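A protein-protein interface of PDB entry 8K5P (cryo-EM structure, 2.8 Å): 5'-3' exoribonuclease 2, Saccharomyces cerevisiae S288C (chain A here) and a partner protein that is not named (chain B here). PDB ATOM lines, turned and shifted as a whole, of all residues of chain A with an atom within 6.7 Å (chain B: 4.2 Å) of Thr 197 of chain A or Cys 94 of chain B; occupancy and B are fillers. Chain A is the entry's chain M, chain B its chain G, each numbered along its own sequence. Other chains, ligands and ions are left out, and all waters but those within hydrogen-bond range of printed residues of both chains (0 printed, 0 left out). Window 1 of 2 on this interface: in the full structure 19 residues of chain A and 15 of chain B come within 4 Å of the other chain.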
ATOM      1  N   ALA A 192     -12.635  23.538  23.674  1.00  0.00           N
ATOM      2  CA  ALA A 192     -13.300  24.483  22.785  1.00  0.00           C
ATOM      3  C   ALA A 192     -14.688  23.990  22.397  1.00  0.00           C
ATOM      4  O   ALA A 192     -15.653  24.765  22.389  1.00  0.00           O
ATOM      5  CB  ALA A 192     -12.447  24.724  21.539  1.00  0.00           C
ATOM      6  N   PHE A 193     -14.810  22.698  22.081  1.00  0.00           N
ATOM      7  CA  PHE A 193     -16.113  22.130  21.755  1.00  0.00           C
ATOM      8  C   PHE A 193     -17.061  22.211  22.944  1.00  0.00           C
ATOM      9  O   PHE A 193     -18.244  22.538  22.785  1.00  0.00           O
ATOM     10  CB  PHE A 193     -15.947  20.681  21.295  1.00  0.00           C
ATOM     11  CG  PHE A 193     -17.233  20.016  20.895  1.00  0.00           C
ATOM     12  CD1 PHE A 193     -17.761  20.205  19.629  1.00  0.00           C
ATOM     13  CD2 PHE A 193     -17.909  19.193  21.781  1.00  0.00           C
ATOM     14  CE1 PHE A 193     -18.942  19.592  19.255  1.00  0.00           C
ATOM     15  CE2 PHE A 193     -19.091  18.578  21.414  1.00  0.00           C
ATOM     16  CZ  PHE A 193     -19.607  18.778  20.150  1.00  0.00           C
ATOM     17  N   LYS A 194     -16.559  21.913  24.145  1.00  0.00           N
ATOM     18  CA  LYS A 194     -17.397  21.992  25.338  1.00  0.00           C
ATOM     19  C   LYS A 194     -17.869  23.419  25.588  1.00  0.00           C
ATOM     20  O   LYS A 194     -19.036  23.643  25.926  1.00  0.00           O
ATOM     21  CB  LYS A 194     -16.636  21.457  26.551  1.00  0.00           C
ATOM     22  CG  LYS A 194     -17.468  20.565  27.457  1.00  0.00           C
ATOM     23  CD  LYS A 194     -18.111  19.429  26.678  1.00  0.00           C
ATOM     24  CE  LYS A 194     -18.946  18.544  27.586  1.00  0.00           C
ATOM     25  NZ  LYS A 194     -18.183  18.107  28.787  1.00  0.00           N
ATOM     26  N   LEU A 195     -16.975  24.398  25.429  1.00  0.00           N
ATOM     27  CA  LEU A 195     -17.361  25.791  25.626  1.00  0.00           C
ATOM     28  C   LEU A 195     -18.374  26.240  24.580  1.00  0.00           C
ATOM     29  O   LEU A 195     -19.311  26.982  24.895  1.00  0.00           O
ATOM     30  CB  LEU A 195     -16.124  26.687  25.593  1.00  0.00           C
ATOM     31  CG  LEU A 195     -15.389  26.871  26.922  1.00  0.00           C
ATOM     32  CD1 LEU A 195     -13.890  26.975  26.698  1.00  0.00           C
ATOM     33  CD2 LEU A 195     -15.911  28.096  27.658  1.00  0.00           C
ATOM     34  N   ALA A 196     -18.204  25.802  23.331  1.00  0.00           N
ATOM     35  CA  ALA A 196     -19.094  26.251  22.265  1.00  0.00           C
ATOM     36  C   ALA A 196     -20.476  25.617  22.379  1.00  0.00           C
ATOM     37  O   ALA A 196     -21.493  26.297  22.193  1.00  0.00           O
ATOM     38  CB  ALA A 196     -18.476  25.945  20.902  1.00  0.00           C
ATOM     39  N   THR A 197     -20.541  24.321  22.685  1.00  0.00           N
ATOM     40  CA  THR A 197     -21.800  23.590  22.635  1.00  0.00           C
ATOM     41  C   THR A 197     -22.570  23.595  23.950  1.00  0.00           C
ATOM     42  O   THR A 197     -23.709  23.118  23.978  1.00  0.00           O
ATOM     43  CB  THR A 197     -21.550  22.139  22.208  1.00  0.00           C
ATOM     44  OG1 THR A 197     -20.659  21.511  23.138  1.00  0.00           O
ATOM     45  CG2 THR A 197     -20.939  22.095  20.817  1.00  0.00           C
ATOM     46  N   ASP A 198     -21.993  24.113  25.030  1.00  0.00           N
ATOM     47  CA  ASP A 198     -22.677  24.120  26.320  1.00  0.00           C
ATOM     48  C   ASP A 198     -23.057  25.543  26.703  1.00  0.00           C
ATOM     49  O   ASP A 198     -22.166  26.371  26.953  1.00  0.00           O
ATOM     50  CB  ASP A 198     -21.797  23.496  27.403  1.00  0.00           C
ATOM     51  CG  ASP A 198     -22.550  22.500  28.262  1.00  0.00           C
ATOM     52  OD1 ASP A 198     -23.764  22.316  28.034  1.00  0.00           O
ATOM     53  OD2 ASP A 198     -21.930  21.902  29.165  1.00  0.00           O
ATOM     54  N   PRO A 199     -24.349  25.879  26.756  1.00  0.00           N
ATOM     55  CA  PRO A 199     -24.738  27.230  27.192  1.00  0.00           C
ATOM     56  C   PRO A 199     -24.358  27.537  28.629  1.00  0.00           C
ATOM     57  O   PRO A 199     -24.219  28.715  28.978  1.00  0.00           O
ATOM     58  CB  PRO A 199     -26.260  27.233  27.003  1.00  0.00           C
ATOM     59  CG  PRO A 199     -26.648  25.797  27.104  1.00  0.00           C
ATOM     60  CD  PRO A 199     -25.518  25.025  26.486  1.00  0.00           C
ATOM     61  N   GLY A 200     -24.186  26.519  29.472  1.00  0.00           N
ATOM     62  CA  GLY A 200     -23.814  26.742  30.856  1.00  0.00           C
ATOM     63  C   GLY A 200     -22.362  27.091  31.083  1.00  0.00           C
ATOM     64  O   GLY A 200     -21.993  27.455  32.204  1.00  0.00           O
ATOM     65  N   LEU A 855     -16.174  31.331  17.990  1.00  0.00           N
ATOM     66  CA  LEU A 855     -16.865  30.854  19.181  1.00  0.00           C
ATOM     67  C   LEU A 855     -15.961  30.814  20.405  1.00  0.00           C
ATOM     68  O   LEU A 855     -16.435  31.040  21.524  1.00  0.00           O
ATOM     69  CB  LEU A 855     -17.438  29.453  18.938  1.00  0.00           C
ATOM     70  CG  LEU A 855     -18.141  29.153  17.611  1.00  0.00           C
ATOM     71  CD1 LEU A 855     -18.914  27.848  17.709  1.00  0.00           C
ATOM     72  CD2 LEU A 855     -19.069  30.285  17.206  1.00  0.00           C
ATOM     73  N   SER B  93     -30.699  25.948  23.782  1.00  0.00           N
ATOM     74  CA  SER B  93     -29.394  25.327  23.624  1.00  0.00           C
ATOM     75  C   SER B  93     -29.382  24.528  22.330  1.00  0.00           C
ATOM     76  O   SER B  93     -30.429  24.132  21.812  1.00  0.00           O
ATOM     77  CB  SER B  93     -29.049  24.424  24.814  1.00  0.00           C
ATOM     78  OG  SER B  93     -27.971  23.559  24.501  1.00  0.00           O
ATOM     79  N   CYS B  94     -28.178  24.295  21.811  1.00  0.00           N
ATOM     80  CA  CYS B  94     -28.008  23.527  20.586  1.00  0.00           C
ATOM     81  C   CYS B  94     -26.701  22.753  20.657  1.00  0.00           C
ATOM     82  O   CYS B  94     -25.713  23.237  21.217  1.00  0.00           O
ATOM     83  CB  CYS B  94     -28.022  24.434  19.349  1.00  0.00           C
ATOM     84  SG  CYS B  94     -27.988  23.542  17.778  1.00  0.00           S
ATOM     85  N   SER B  95     -26.706  21.552  20.087  1.00  0.00           N
ATOM     86  CA  SER B  95     -25.529  20.693  20.056  1.00  0.00           C
ATOM     87  C   SER B  95     -25.714  19.678  18.936  1.00  0.00           C
ATOM     88  O   SER B  95     -26.696  19.720  18.188  1.00  0.00           O
ATOM     89  CB  SER B  95     -25.305  20.009  21.408  1.00  0.00           C
ATOM     90  OG  SER B  95     -24.185  19.141  21.370  1.00  0.00           O
ATOM     91  N   GLY B  98     -28.940  17.608  19.426  1.00  0.00           N
ATOM     92  CA  GLY B  98     -30.180  18.238  19.017  1.00  0.00           C
ATOM     93  C   GLY B  98     -30.266  19.645  19.581  1.00  0.00           C
ATOM     94  O   GLY B  98     -29.272  20.210  20.031  1.00  0.00           O
ATOM     95  N   PHE B 121     -25.758  19.585  11.195  1.00  0.00           N
ATOM     96  CA  PHE B 121     -25.082  20.343  12.237  1.00  0.00           C
ATOM     97  C   PHE B 121     -23.838  21.026  11.685  1.00  0.00           C
ATOM     98  O   PHE B 121     -23.043  20.417  10.963  1.00  0.00           O
ATOM     99  CB  PHE B 121     -24.703  19.430  13.402  1.00  0.00           C
ATOM    100  CG  PHE B 121     -24.251  20.167  14.630  1.00  0.00           C
ATOM    101  CD1 PHE B 121     -25.013  21.199  15.153  1.00  0.00           C
ATOM    102  CD2 PHE B 121     -23.067  19.827  15.262  1.00  0.00           C
ATOM    103  CE1 PHE B 121     -24.600  21.880  16.283  1.00  0.00           C
ATOM    104  CE2 PHE B 121     -22.650  20.504  16.393  1.00  0.00           C
ATOM    105  CZ  PHE B 121     -23.417  21.531  16.904  1.00  0.00           C
ATOM    106  N   PRO B 128     -23.959  28.099  17.014  1.00  0.00           N
ATOM    107  CA  PRO B 128     -23.949  26.732  16.467  1.00  0.00           C
ATOM    108  C   PRO B 128     -25.371  26.254  16.220  1.00  0.00           C
ATOM    109  O   PRO B 128     -26.164  26.100  17.152  1.00  0.00           O
ATOM    110  CB  PRO B 128     -23.252  25.915  17.562  1.00  0.00           C
ATOM    111  CG  PRO B 128     -23.368  26.741  18.803  1.00  0.00           C
ATOM    112  CD  PRO B 128     -23.366  28.169  18.359  1.00  0.00           C
ATOM    113  N   SER B 129     -25.693  26.024  14.950  1.00  0.00           N
ATOM    114  CA  SER B 129     -27.072  25.790  14.550  1.00  0.00           C
ATOM    115  C   SER B 129     -27.137  24.761  13.430  1.00  0.00           C
ATOM    116  O   SER B 129     -26.171  24.561  12.689  1.00  0.00           O
ATOM    117  CB  SER B 129     -27.738  27.092  14.092  1.00  0.00           C
ATOM    118  OG  SER B 129     -27.753  28.050  15.136  1.00  0.00           O
ATOM    119  N   TYR B 130     -28.294  24.114  13.321  1.00  0.00           N
ATOM    120  CA  TYR B 130     -28.582  23.228  12.201  1.00  0.00           C
ATOM    121  C   TYR B 130     -29.038  24.067  11.014  1.00  0.00           C
ATOM    122  O   TYR B 130     -30.061  24.756  11.093  1.00  0.00           O
ATOM    123  CB  TYR B 130     -29.654  22.212  12.586  1.00  0.00           C
ATOM    124  CG  TYR B 130     -29.214  21.198  13.617  1.00  0.00           C
ATOM    125  CD1 TYR B 130     -28.517  20.057  13.243  1.00  0.00           C
ATOM    126  CD2 TYR B 130     -29.494  21.383  14.965  1.00  0.00           C
ATOM    127  CE1 TYR B 130     -28.115  19.126  14.182  1.00  0.00           C
ATOM    128  CE2 TYR B 130     -29.094  20.459  15.911  1.00  0.00           C
ATOM    129  CZ  TYR B 130     -28.404  19.333  15.514  1.00  0.00           C
ATOM    130  OH  TYR B 130     -28.003  18.409  16.450  1.00  0.00           O
ATOM    131  N   ILE B 139     -29.902  29.642  18.323  1.00  0.00           N
ATOM    132  CA  ILE B 139     -29.979  29.602  19.781  1.00  0.00           C
ATOM    133  C   ILE B 139     -31.284  30.223  20.264  1.00  0.00           C
ATOM    134  O   ILE B 139     -31.950  29.686  21.157  1.00  0.00           O
ATOM    135  CB  ILE B 139     -28.752  30.299  20.399  1.00  0.00           C
ATOM    136  CG1 ILE B 139     -27.506  29.426  20.235  1.00  0.00           C
ATOM    137  CG2 ILE B 139     -28.991  30.621  21.868  1.00  0.00           C
ATOM    138  CD1 ILE B 139     -27.672  28.019  20.764  1.00  0.00           C
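O of Thr 197 of chain A sits close to O of Cys 94 of chain B (3.4 Å).
The side-chain sulfur of Cys 94 of chain B lies within hydrogen-bond range of the backbone carbonyl oxygen of Pro 128 of chain B (3.2 Å).
OG1 of Thr 197 of chain A lies within hydrogen-bond range of O of Phe 193 of chain A.
Among the printed residues, merely in contact across the chains: Ala 196 of chain A with Pro 128 of chain B (3.9 Å) and Pro 199 of chain A with Ser 93 of chain B (3.5 Å).
Thr 197 of chain A touches just one residue of chain B: Cys 94 (3.4 Å).
Of the printed residues of chain B, Pro 199 of chain A touches Ser 93 (3.5 Å).
Of the printed residues of chain A, Ser 93 of chain B touches Pro 199.
Cys 94 of chain B touches one residue of chain A.
The nearest residue of chain B that does not touch Thr 197 of chain A is Ser 95 of chain B (4.1 Å).
The nearest residue of chain A that does not touch Cys 94 of chain B is Ala 196 of chain A (5.3 Å).
The nearest printed residue of chain A that does not touch Pro 128 of chain B is Leu 855 of chain A (4.5 Å).
Of the 9 printed residues of chain B, 3 touch a printed residue of chain A.
Hydrophobic or aromatic side chains of chain B that line the printed part of chain A: Pro 128.
Of the 10 printed residues of chain A, 3 touch a printed residue of chain B.
Among the printed residues, 3 pairs touch across the chains.
Among the printed residues, no Asp or Glu carboxylate lies within 4 Å of a Lys or Arg side-chain nitrogen of the other chain.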
